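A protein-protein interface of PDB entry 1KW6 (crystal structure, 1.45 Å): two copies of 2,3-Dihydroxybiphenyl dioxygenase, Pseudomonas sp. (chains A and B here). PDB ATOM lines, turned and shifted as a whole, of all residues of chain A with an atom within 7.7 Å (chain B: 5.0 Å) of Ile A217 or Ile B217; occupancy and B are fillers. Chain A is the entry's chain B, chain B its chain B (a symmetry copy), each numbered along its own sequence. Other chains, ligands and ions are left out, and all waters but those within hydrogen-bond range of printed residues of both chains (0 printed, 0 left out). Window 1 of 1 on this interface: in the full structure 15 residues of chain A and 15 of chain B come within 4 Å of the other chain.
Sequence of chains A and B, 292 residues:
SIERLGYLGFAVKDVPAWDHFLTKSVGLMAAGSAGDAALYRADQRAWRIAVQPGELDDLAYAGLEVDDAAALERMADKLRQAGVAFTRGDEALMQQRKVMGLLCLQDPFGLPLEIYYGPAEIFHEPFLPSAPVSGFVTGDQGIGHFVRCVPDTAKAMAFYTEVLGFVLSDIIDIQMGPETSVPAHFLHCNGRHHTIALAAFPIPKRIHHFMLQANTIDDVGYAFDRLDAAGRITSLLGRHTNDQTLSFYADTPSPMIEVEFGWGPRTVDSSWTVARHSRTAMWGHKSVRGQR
The indole nitrogen (NE1) of Trp A283 sits at hydrogen-bond distance from the side-chain carboxylate (OD2) of Asp B218.
NH2 of Arg A239 is in salt-bridge range of OD2 of Asp B218 (2.9 Å).
NH2 of Arg B239 is in salt-bridge range of OD2 of Asp A218, 2.9 Å away.
The side-chain carboxylate (OD2) of Asp A218 lies within hydrogen-bond range of the indole nitrogen (NE1) of Trp B283, at 2.9 Å.
The backbone carbonyl oxygen (O) of Leu A246 lies within hydrogen-bond range of the backbone NH (N) of Trp A263 (2.8 Å).
The backbone carbonyl oxygen (O) of Arg A239 is in hydrogen-bond range of the backbone NH (N) of Met A282.
N of Trp B263 sits at hydrogen-bond distance from O of Leu B246, at 2.8 Å.
The guanidinium group (NH1) of Arg A239 lies within hydrogen-bond range of the backbone carbonyl oxygen (O) of Gly A264, at 3.0 Å.
The backbone NH of Arg B239 lies within hydrogen-bond range of the backbone carbonyl oxygen of Trp B283, at 2.9 Å.
N of Arg A239 lies within hydrogen-bond range of O of Trp A283.
Ile A217 touches Ile B217 (CD1 to CD1, 3.8 Å).
NH2 of Arg B239 touches CG2 of Ile A217, 3.5 Å away.
CG1 of Ile A217 touches CD1 of Leu B246 (3.997 Å).
Gly A221 touches Trp B283 (CA to CD2, 3.4 Å).
Trp B283 touches Tyr A222.
Leu A237 touches Trp B283.
Ile B217 touches Arg A239 (CG2 to NH2, 3.5 Å).
CD1 of Leu A246 touches CG1 of Ile B217, 3.996 Å away.
CE of Met A282 touches OD1 of Asp B218, at 3.8 Å.
CA of Gly B221 touches CD2 of Trp A283 (3.4 Å).
Printed residues of chain B within 4 Å of Ile A217: Ile B217, Arg B239 and Leu B246.
Of the printed residues of chain A, Ile B217 touches Ile A217, Arg A239 and Leu A246.
Of the printed residues of chain A, Leu B246 touches Ile A217.
Of the printed residues of chain B, Gly A221 touches Trp B283 (3.4 Å).
Of the printed residues of chain B, Asp A218 touches Arg B239 (2.9 Å) and Trp B283 (2.9 Å).
Of the printed residues of chain B, Leu A237 touches Trp B283 (3.8 Å).
The nearest printed residue of chain B that does not touch Ile A217 is Trp B283 (4.3 Å).
Of the 23 printed residues of chain A, 9 touch a printed residue of chain B.
Hydrophobic or aromatic side chains of chain A that line the printed part of chain B: Ile A217, Tyr A222, Leu A237, Leu A246, Met A282 and Trp A283.
Among the printed residues, Asp or Glu carboxylates within 4 Å of a Lys or Arg side-chain nitrogen of the other chain: Asp A218 with Arg B239 and Arg A239 with Asp B218.
Ile A217 touches its own counterpart, Ile B217.
Asp A218 touches Arg B239, and with the chains exchanged Arg A239 touches Asp B218.
Asp A218 touches Trp B283, and with the chains exchanged Trp A283 touches Asp B218.
Gly A221 touches Trp B283, and with the chains exchanged Trp A283 touches Gly B221.
Positions printed for both chains: 215, 216, 217, 218, 219, 220, 221, 239, 246, 263 and 283.
Of the 14 pairs that touch across the chains among the printed residues, 11 have their exchanged pair printed and touching as well.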
ATOM      1  N   SER A 134      18.315  19.169  16.111  1.00  0.00           N
ATOM      2  CA  SER A 134      17.423  19.758  15.114  1.00  0.00           C
ATOM      3  C   SER A 134      16.407  20.755  15.682  1.00  0.00           C
ATOM      4  O   SER A 134      15.857  21.582  14.941  1.00  0.00           O
ATOM      5  CB  SER A 134      16.737  18.651  14.341  1.00  0.00           C
ATOM      6  OG  SER A 134      15.661  18.078  15.072  1.00  0.00           O
ATOM      7  N   ALA A 214      13.717  16.614  22.414  1.00  0.00           N
ATOM      8  CA  ALA A 214      14.211  16.977  21.087  1.00  0.00           C
ATOM      9  C   ALA A 214      13.251  16.482  20.010  1.00  0.00           C
ATOM     10  O   ALA A 214      12.435  15.603  20.233  1.00  0.00           O
ATOM     11  CB  ALA A 214      15.592  16.417  20.860  1.00  0.00           C
ATOM     12  N   ASN A 215      13.403  17.022  18.804  1.00  0.00           N
ATOM     13  CA  ASN A 215      12.489  16.707  17.712  1.00  0.00           C
ATOM     14  C   ASN A 215      12.626  15.306  17.115  1.00  0.00           C
ATOM     15  O   ASN A 215      11.631  14.743  16.640  1.00  0.00           O
ATOM     16  CB  ASN A 215      12.682  17.706  16.569  1.00  0.00           C
ATOM     17  CG  ASN A 215      12.152  19.086  16.877  1.00  0.00           C
ATOM     18  OD1 ASN A 215      11.358  19.282  17.797  1.00  0.00           O
ATOM     19  ND2 ASN A 215      12.603  20.067  16.097  1.00  0.00           N
ATOM     20  N   THR A 216      13.842  14.749  17.093  1.00  0.00           N
ATOM     21  CA  THR A 216      14.053  13.446  16.452  1.00  0.00           C
ATOM     22  C   THR A 216      14.800  12.422  17.302  1.00  0.00           C
ATOM     23  O   THR A 216      15.497  12.770  18.254  1.00  0.00           O
ATOM     24  CB  THR A 216      14.812  13.586  15.105  1.00  0.00           C
ATOM     25  OG1 THR A 216      16.190  13.928  15.336  1.00  0.00           O
ATOM     26  CG2 THR A 216      14.249  14.713  14.253  1.00  0.00           C
ATOM     27  N   ILE A 217      14.672  11.153  16.919  1.00  0.00           N
ATOM     28  CA  ILE A 217      15.383  10.071  17.598  1.00  0.00           C
ATOM     29  C   ILE A 217      16.898  10.266  17.425  1.00  0.00           C
ATOM     30  O   ILE A 217      17.671  10.014  18.352  1.00  0.00           O
ATOM     31  CB  ILE A 217      14.910   8.685  17.069  1.00  0.00           C
ATOM     32  CG1 ILE A 217      15.620   7.510  17.732  1.00  0.00           C
ATOM     33  CG2 ILE A 217      15.194   8.511  15.622  1.00  0.00           C
ATOM     34  CD1 ILE A 217      14.793   6.791  18.796  1.00  0.00           C
ATOM     35  N   ASP A 218      17.322  10.727  16.248  1.00  0.00           N
ATOM     36  CA  ASP A 218      18.738  10.970  16.011  1.00  0.00           C
ATOM     37  C   ASP A 218      19.264  12.084  16.921  1.00  0.00           C
ATOM     38  O   ASP A 218      20.414  12.045  17.357  1.00  0.00           O
ATOM     39  CB  ASP A 218      19.016  11.276  14.535  1.00  0.00           C
ATOM     40  CG  ASP A 218      18.889  10.059  13.661  1.00  0.00           C
ATOM     41  OD1 ASP A 218      18.545  10.229  12.453  1.00  0.00           O
ATOM     42  OD2 ASP A 218      19.090   8.908  14.078  1.00  0.00           O
ATOM     43  N   ASP A 219      18.434  13.078  17.204  1.00  0.00           N
ATOM     44  CA  ASP A 219      18.859  14.130  18.128  1.00  0.00           C
ATOM     45  C   ASP A 219      19.258  13.480  19.450  1.00  0.00           C
ATOM     46  O   ASP A 219      20.271  13.827  20.049  1.00  0.00           O
ATOM     47  CB  ASP A 219      17.728  15.119  18.401  1.00  0.00           C
ATOM     48  CG  ASP A 219      17.457  16.059  17.245  1.00  0.00           C
ATOM     49  OD1 ASP A 219      16.304  16.547  17.167  1.00  0.00           O
ATOM     50  OD2 ASP A 219      18.344  16.408  16.429  1.00  0.00           O
ATOM     51  N   VAL A 220      18.448  12.532  19.904  1.00  0.00           N
ATOM     52  CA  VAL A 220      18.706  11.854  21.169  1.00  0.00           C
ATOM     53  C   VAL A 220      19.970  10.981  21.076  1.00  0.00           C
ATOM     54  O   VAL A 220      20.828  11.019  21.953  1.00  0.00           O
ATOM     55  CB  VAL A 220      17.486  11.025  21.614  1.00  0.00           C
ATOM     56  CG1 VAL A 220      17.777  10.293  22.905  1.00  0.00           C
ATOM     57  CG2 VAL A 220      16.273  11.914  21.806  1.00  0.00           C
ATOM     58  N   GLY A 221      20.093  10.211  20.001  1.00  0.00           N
ATOM     59  CA  GLY A 221      21.258   9.360  19.811  1.00  0.00           C
ATOM     60  C   GLY A 221      22.557  10.139  19.751  1.00  0.00           C
ATOM     61  O   GLY A 221      23.559   9.743  20.367  1.00  0.00           O
ATOM     62  N   TYR A 222      22.562  11.233  18.999  1.00  0.00           N
ATOM     63  CA  TYR A 222      23.739  12.074  18.907  1.00  0.00           C
ATOM     64  C   TYR A 222      24.069  12.701  20.267  1.00  0.00           C
ATOM     65  O   TYR A 222      25.241  12.767  20.648  1.00  0.00           O
ATOM     66  CB  TYR A 222      23.528  13.154  17.864  1.00  0.00           C
ATOM     67  CG  TYR A 222      23.699  12.748  16.417  1.00  0.00           C
ATOM     68  CD1 TYR A 222      22.748  13.095  15.470  1.00  0.00           C
ATOM     69  CD2 TYR A 222      24.834  12.079  15.985  1.00  0.00           C
ATOM     70  CE1 TYR A 222      22.919  12.778  14.138  1.00  0.00           C
ATOM     71  CE2 TYR A 222      25.013  11.758  14.643  1.00  0.00           C
ATOM     72  CZ  TYR A 222      24.051  12.109  13.735  1.00  0.00           C
ATOM     73  OH  TYR A 222      24.244  11.834  12.389  1.00  0.00           O
ATOM     74  N   ALA A 223      23.059  13.176  20.995  1.00  0.00           N
ATOM     75  CA  ALA A 223      23.278  13.776  22.314  1.00  0.00           C
ATOM     76  C   ALA A 223      23.861  12.754  23.284  1.00  0.00           C
ATOM     77  O   ALA A 223      24.697  13.102  24.118  1.00  0.00           O
ATOM     78  CB  ALA A 223      22.004  14.361  22.872  1.00  0.00           C
ATOM     79  N   PHE A 224      23.430  11.502  23.190  1.00  0.00           N
ATOM     80  CA  PHE A 224      23.978  10.470  24.060  1.00  0.00           C
ATOM     81  C   PHE A 224      25.488  10.379  23.890  1.00  0.00           C
ATOM     82  O   PHE A 224      26.234  10.301  24.868  1.00  0.00           O
ATOM     83  CB  PHE A 224      23.335   9.117  23.733  1.00  0.00           C
ATOM     84  CG  PHE A 224      23.794   8.002  24.626  1.00  0.00           C
ATOM     85  CD1 PHE A 224      24.974   7.326  24.368  1.00  0.00           C
ATOM     86  CD2 PHE A 224      23.038   7.623  25.718  1.00  0.00           C
ATOM     87  CE1 PHE A 224      25.406   6.309  25.198  1.00  0.00           C
ATOM     88  CE2 PHE A 224      23.452   6.605  26.544  1.00  0.00           C
ATOM     89  CZ  PHE A 224      24.637   5.941  26.284  1.00  0.00           C
ATOM     90  N   LEU A 237      20.075   4.324  26.836  1.00  0.00           N
ATOM     91  CA  LEU A 237      18.838   4.667  26.159  1.00  0.00           C
ATOM     92  C   LEU A 237      17.714   3.745  26.644  1.00  0.00           C
ATOM     93  O   LEU A 237      17.929   2.562  26.936  1.00  0.00           O
ATOM     94  CB  LEU A 237      19.004   4.524  24.643  1.00  0.00           C
ATOM     95  CG  LEU A 237      19.857   5.605  23.977  1.00  0.00           C
ATOM     96  CD1 LEU A 237      20.254   5.217  22.565  1.00  0.00           C
ATOM     97  CD2 LEU A 237      19.115   6.936  23.993  1.00  0.00           C
ATOM     98  N   GLY A 238      16.507   4.274  26.733  1.00  0.00           N
ATOM     99  CA  GLY A 238      15.358   3.492  27.151  1.00  0.00           C
ATOM    100  C   GLY A 238      14.102   4.243  26.822  1.00  0.00           C
ATOM    101  O   GLY A 238      14.143   5.348  26.286  1.00  0.00           O
ATOM    102  N   ARG A 239      12.969   3.632  27.150  1.00  0.00           N
ATOM    103  CA  ARG A 239      11.685   4.237  26.880  1.00  0.00           C
ATOM    104  C   ARG A 239      10.804   4.038  28.110  1.00  0.00           C
ATOM    105  O   ARG A 239      10.765   2.947  28.670  1.00  0.00           O
ATOM    106  CB  ARG A 239      11.075   3.592  25.647  1.00  0.00           C
ATOM    107  CG  ARG A 239       9.979   4.411  25.043  1.00  0.00           C
ATOM    108  CD  ARG A 239       9.576   3.984  23.655  1.00  0.00           C
ATOM    109  NE  ARG A 239       8.961   5.101  22.963  1.00  0.00           N
ATOM    110  CZ  ARG A 239       8.728   5.126  21.675  1.00  0.00           C
ATOM    111  NH1 ARG A 239       8.189   6.212  21.139  1.00  0.00           N
ATOM    112  NH2 ARG A 239       9.033   4.074  20.922  1.00  0.00           N
ATOM    113  N   LEU A 246      11.342   8.225  24.733  1.00  0.00           N
ATOM    114  CA  LEU A 246      12.590   7.493  24.511  1.00  0.00           C
ATOM    115  C   LEU A 246      13.718   8.465  24.882  1.00  0.00           C
ATOM    116  O   LEU A 246      13.876   9.507  24.257  1.00  0.00           O
ATOM    117  CB  LEU A 246      12.695   7.073  23.046  1.00  0.00           C
ATOM    118  CG  LEU A 246      13.666   5.937  22.732  1.00  0.00           C
ATOM    119  CD1 LEU A 246      13.407   5.399  21.341  1.00  0.00           C
ATOM    120  CD2 LEU A 246      15.098   6.376  22.856  1.00  0.00           C
ATOM    121  N   SER A 247      14.487   8.141  25.919  1.00  0.00           N
ATOM    122  CA  SER A 247      15.458   9.084  26.454  1.00  0.00           C
ATOM    123  C   SER A 247      16.655   8.406  27.073  1.00  0.00           C
ATOM    124  O   SER A 247      16.719   7.186  27.202  1.00  0.00           O
ATOM    125  CB  SER A 247      14.809   9.899  27.579  1.00  0.00           C
ATOM    126  OG  SER A 247      14.526   9.056  28.702  1.00  0.00           O
ATOM    127  N   PHE A 261      17.214  13.649  28.339  1.00  0.00           N
ATOM    128  CA  PHE A 261      17.171  14.146  26.967  1.00  0.00           C
ATOM    129  C   PHE A 261      16.401  13.088  26.183  1.00  0.00           C
ATOM    130  O   PHE A 261      16.829  11.948  26.095  1.00  0.00           O
ATOM    131  CB  PHE A 261      18.599  14.340  26.459  1.00  0.00           C
ATOM    132  CG  PHE A 261      18.720  15.118  25.169  1.00  0.00           C
ATOM    133  CD1 PHE A 261      19.269  16.392  25.163  1.00  0.00           C
ATOM    134  CD2 PHE A 261      18.332  14.565  23.968  1.00  0.00           C
ATOM    135  CE1 PHE A 261      19.402  17.102  23.980  1.00  0.00           C
ATOM    136  CE2 PHE A 261      18.474  15.269  22.779  1.00  0.00           C
ATOM    137  CZ  PHE A 261      19.013  16.535  22.795  1.00  0.00           C
ATOM    138  N   GLY A 262      15.245  13.458  25.641  1.00  0.00           N
ATOM    139  CA  GLY A 262      14.347  12.463  25.074  1.00  0.00           C
ATOM    140  C   GLY A 262      13.566  12.868  23.843  1.00  0.00           C
ATOM    141  O   GLY A 262      13.666  14.009  23.377  1.00  0.00           O
ATOM    142  N   TRP A 263      12.774  11.919  23.351  1.00  0.00           N
ATOM    143  CA  TRP A 263      12.011  12.048  22.116  1.00  0.00           C
ATOM    144  C   TRP A 263      10.753  11.184  22.125  1.00  0.00           C
ATOM    145  O   TRP A 263      10.696  10.164  22.796  1.00  0.00           O
ATOM    146  CB  TRP A 263      12.870  11.528  20.953  1.00  0.00           C
ATOM    147  CG  TRP A 263      12.121  11.332  19.680  1.00  0.00           C
ATOM    148  CD1 TRP A 263      11.794  12.297  18.773  1.00  0.00           C
ATOM    149  CD2 TRP A 263      11.600  10.101  19.162  1.00  0.00           C
ATOM    150  NE1 TRP A 263      11.093  11.747  17.730  1.00  0.00           N
ATOM    151  CE2 TRP A 263      10.961  10.399  17.941  1.00  0.00           C
ATOM    152  CE3 TRP A 263      11.611   8.771  19.601  1.00  0.00           C
ATOM    153  CZ2 TRP A 263      10.349   9.421  17.158  1.00  0.00           C
ATOM    154  CZ3 TRP A 263      10.994   7.802  18.822  1.00  0.00           C
ATOM    155  CH2 TRP A 263      10.375   8.134  17.618  1.00  0.00           C
ATOM    156  N   GLY A 264       9.741  11.603  21.370  1.00  0.00           N
ATOM    157  CA  GLY A 264       8.662  10.707  20.966  1.00  0.00           C
ATOM    158  C   GLY A 264       7.643  10.137  21.926  1.00  0.00           C
ATOM    159  O   GLY A 264       7.192   9.005  21.732  1.00  0.00           O
ATOM    160  N   MET A 282       9.737   0.756  30.032  1.00  0.00           N
ATOM    161  CA  MET A 282       9.198  -0.395  29.305  1.00  0.00           C
ATOM    162  C   MET A 282      10.390  -1.217  28.780  1.00  0.00           C
ATOM    163  O   MET A 282      10.330  -2.451  28.733  1.00  0.00           O
ATOM    164  CB  MET A 282       8.237   0.014  28.177  1.00  0.00           C
ATOM    165  CG  MET A 282       8.743   1.041  27.203  1.00  0.00           C
ATOM    166  SD  MET A 282       7.427   1.717  26.103  1.00  0.00           S
ATOM    167  CE  MET A 282       7.283   0.416  24.966  1.00  0.00           C
ATOM    168  N   TRP A 283      11.458  -0.526  28.369  1.00  0.00           N
ATOM    169  CA  TRP A 283      12.710  -1.160  27.973  1.00  0.00           C
ATOM    170  C   TRP A 283      13.859  -0.183  28.193  1.00  0.00           C
ATOM    171  O   TRP A 283      13.656   1.029  28.234  1.00  0.00           O
ATOM    172  CB  TRP A 283      12.696  -1.686  26.526  1.00  0.00           C
ATOM    173  CG  TRP A 283      12.359  -0.718  25.420  1.00  0.00           C
ATOM    174  CD1 TRP A 283      11.165  -0.610  24.762  1.00  0.00           C
ATOM    175  CD2 TRP A 283      13.246   0.210  24.771  1.00  0.00           C
ATOM    176  NE1 TRP A 283      11.245   0.350  23.785  1.00  0.00           N
ATOM    177  CE2 TRP A 283      12.516   0.854  23.755  1.00  0.00           C
ATOM    178  CE3 TRP A 283      14.594   0.553  24.940  1.00  0.00           C
ATOM    179  CZ2 TRP A 283      13.077   1.814  22.934  1.00  0.00           C
ATOM    180  CZ3 TRP A 283      15.151   1.501  24.104  1.00  0.00           C
ATOM    181  CH2 TRP A 283      14.388   2.126  23.126  1.00  0.00           C
ATOM    182  N   ASN B 215       9.978  -4.794  12.818  1.00  0.00           N
ATOM    183  CA  ASN B 215       9.076  -3.760  12.327  1.00  0.00           C
ATOM    184  C   ASN B 215       9.117  -2.429  13.080  1.00  0.00           C
ATOM    185  O   ASN B 215       8.875  -1.375  12.476  1.00  0.00           O
ATOM    186  CB  ASN B 215       7.632  -4.263  12.379  1.00  0.00           C
ATOM    187  CG  ASN B 215       7.318  -5.308  11.337  1.00  0.00           C
ATOM    188  OD1 ASN B 215       8.039  -5.476  10.353  1.00  0.00           O
ATOM    189  ND2 ASN B 215       6.223  -6.034  11.556  1.00  0.00           N
ATOM    190  N   THR B 216       9.381  -2.458  14.391  1.00  0.00           N
ATOM    191  CA  THR B 216       9.346  -1.224  15.185  1.00  0.00           C
ATOM    192  C   THR B 216      10.575  -0.983  16.057  1.00  0.00           C
ATOM    193  O   THR B 216      11.328  -1.905  16.369  1.00  0.00           O
ATOM    194  CB  THR B 216       8.096  -1.170  16.105  1.00  0.00           C
ATOM    195  OG1 THR B 216       8.225  -2.109  17.187  1.00  0.00           O
ATOM    196  CG2 THR B 216       6.831  -1.573  15.364  1.00  0.00           C
ATOM    197  N   ILE B 217      10.746   0.269  16.478  1.00  0.00           N
ATOM    198  CA  ILE B 217      11.842   0.636  17.373  1.00  0.00           C
ATOM    199  C   ILE B 217      11.670  -0.092  18.716  1.00  0.00           C
ATOM    200  O   ILE B 217      12.651  -0.534  19.318  1.00  0.00           O
ATOM    201  CB  ILE B 217      11.913   2.180  17.552  1.00  0.00           C
ATOM    202  CG1 ILE B 217      13.033   2.630  18.484  1.00  0.00           C
ATOM    203  CG2 ILE B 217      10.681   2.729  18.173  1.00  0.00           C
ATOM    204  CD1 ILE B 217      14.261   3.191  17.770  1.00  0.00           C
ATOM    205  N   ASP B 218      10.428  -0.229  19.181  1.00  0.00           N
ATOM    206  CA  ASP B 218      10.174  -0.932  20.430  1.00  0.00           C
ATOM    207  C   ASP B 218      10.563  -2.409  20.318  1.00  0.00           C
ATOM    208  O   ASP B 218      11.027  -3.009  21.288  1.00  0.00           O
ATOM    209  CB  ASP B 218       8.717  -0.771  20.879  1.00  0.00           C
ATOM    210  CG  ASP B 218       8.419   0.614  21.384  1.00  0.00           C
ATOM    211  OD1 ASP B 218       7.236   1.049  21.260  1.00  0.00           O
ATOM    212  OD2 ASP B 218       9.283   1.343  21.894  1.00  0.00           O
ATOM    213  N   ASP B 219      10.374  -2.999  19.147  1.00  0.00           N
ATOM    214  CA  ASP B 219      10.798  -4.387  18.963  1.00  0.00           C
ATOM    215  C   ASP B 219      12.286  -4.484  19.286  1.00  0.00           C
ATOM    216  O   ASP B 219      12.733  -5.409  19.957  1.00  0.00           O
ATOM    217  CB  ASP B 219      10.588  -4.845  17.521  1.00  0.00           C
ATOM    218  CG  ASP B 219       9.136  -5.103  17.176  1.00  0.00           C
ATOM    219  OD1 ASP B 219       8.813  -5.006  15.968  1.00  0.00           O
ATOM    220  OD2 ASP B 219       8.288  -5.467  18.026  1.00  0.00           O
ATOM    221  N   VAL B 220      13.056  -3.520  18.796  1.00  0.00           N
ATOM    222  CA  VAL B 220      14.498  -3.516  19.012  1.00  0.00           C
ATOM    223  C   VAL B 220      14.829  -3.275  20.496  1.00  0.00           C
ATOM    224  O   VAL B 220      15.649  -3.977  21.081  1.00  0.00           O
ATOM    225  CB  VAL B 220      15.192  -2.479  18.109  1.00  0.00           C
ATOM    226  CG1 VAL B 220      16.681  -2.451  18.369  1.00  0.00           C
ATOM    227  CG2 VAL B 220      14.946  -2.790  16.646  1.00  0.00           C
ATOM    228  N   GLY B 221      14.176  -2.294  21.109  1.00  0.00           N
ATOM    229  CA  GLY B 221      14.406  -1.996  22.514  1.00  0.00           C
ATOM    230  C   GLY B 221      14.086  -3.163  23.426  1.00  0.00           C
ATOM    231  O   GLY B 221      14.854  -3.468  24.353  1.00  0.00           O
ATOM    232  N   ARG B 239      23.085   3.577  15.516  1.00  0.00           N
ATOM    233  CA  ARG B 239      22.534   3.700  14.186  1.00  0.00           C
ATOM    234  C   ARG B 239      23.697   3.787  13.201  1.00  0.00           C
ATOM    235  O   ARG B 239      24.654   4.513  13.442  1.00  0.00           O
ATOM    236  CB  ARG B 239      21.652   4.935  14.119  1.00  0.00           C
ATOM    237  CG  ARG B 239      20.717   4.921  12.953  1.00  0.00           C
ATOM    238  CD  ARG B 239      19.613   5.944  13.028  1.00  0.00           C
ATOM    239  NE  ARG B 239      18.494   5.513  12.210  1.00  0.00           N
ATOM    240  CZ  ARG B 239      17.303   6.053  12.256  1.00  0.00           C
ATOM    241  NH1 ARG B 239      16.343   5.561  11.486  1.00  0.00           N
ATOM    242  NH2 ARG B 239      17.066   7.078  13.068  1.00  0.00           N
ATOM    243  N   LEU B 246      18.918   1.279  12.883  1.00  0.00           N
ATOM    244  CA  LEU B 246      19.073   1.455  14.327  1.00  0.00           C
ATOM    245  C   LEU B 246      19.058   0.043  14.926  1.00  0.00           C
ATOM    246  O   LEU B 246      18.065  -0.668  14.825  1.00  0.00           O
ATOM    247  CB  LEU B 246      17.918   2.291  14.878  1.00  0.00           C
ATOM    248  CG  LEU B 246      18.145   2.953  16.236  1.00  0.00           C
ATOM    249  CD1 LEU B 246      17.091   4.010  16.482  1.00  0.00           C
ATOM    250  CD2 LEU B 246      18.139   1.949  17.354  1.00  0.00           C
ATOM    251  N   TRP B 263      16.196  -1.904  13.141  1.00  0.00           N
ATOM    252  CA  TRP B 263      14.986  -1.252  12.657  1.00  0.00           C
ATOM    253  C   TRP B 263      15.297  -0.012  11.822  1.00  0.00           C
ATOM    254  O   TRP B 263      16.326   0.623  11.999  1.00  0.00           O
ATOM    255  CB  TRP B 263      14.181  -0.753  13.866  1.00  0.00           C
ATOM    256  CG  TRP B 263      13.072   0.179  13.520  1.00  0.00           C
ATOM    257  CD1 TRP B 263      11.833  -0.166  13.063  1.00  0.00           C
ATOM    258  CD2 TRP B 263      13.086   1.611  13.597  1.00  0.00           C
ATOM    259  NE1 TRP B 263      11.081   0.960  12.840  1.00  0.00           N
ATOM    260  CE2 TRP B 263      11.825   2.065  13.162  1.00  0.00           C
ATOM    261  CE3 TRP B 263      14.036   2.560  13.996  1.00  0.00           C
ATOM    262  CZ2 TRP B 263      11.490   3.418  13.120  1.00  0.00           C
ATOM    263  CZ3 TRP B 263      13.700   3.906  13.944  1.00  0.00           C
ATOM    264  CH2 TRP B 263      12.441   4.318  13.512  1.00  0.00           C
ATOM    265  N   TRP B 283      25.847   7.239  15.386  1.00  0.00           N
ATOM    266  CA  TRP B 283      25.803   7.396  16.835  1.00  0.00           C
ATOM    267  C   TRP B 283      25.650   6.024  17.483  1.00  0.00           C
ATOM    268  O   TRP B 283      25.177   5.080  16.853  1.00  0.00           O
ATOM    269  CB  TRP B 283      24.704   8.362  17.312  1.00  0.00           C
ATOM    270  CG  TRP B 283      23.284   8.090  16.887  1.00  0.00           C
ATOM    271  CD1 TRP B 283      22.588   8.730  15.898  1.00  0.00           C
ATOM    272  CD2 TRP B 283      22.349   7.181  17.494  1.00  0.00           C
ATOM    273  NE1 TRP B 283      21.306   8.247  15.828  1.00  0.00           N
ATOM    274  CE2 TRP B 283      21.126   7.311  16.808  1.00  0.00           C
ATOM    275  CE3 TRP B 283      22.419   6.277  18.561  1.00  0.00           C
ATOM    276  CZ2 TRP B 283      20.008   6.571  17.143  1.00  0.00           C
ATOM    277  CZ3 TRP B 283      21.292   5.554  18.900  1.00  0.00           C
ATOM    278  CH2 TRP B 283      20.110   5.700  18.183  1.00  0.00           C
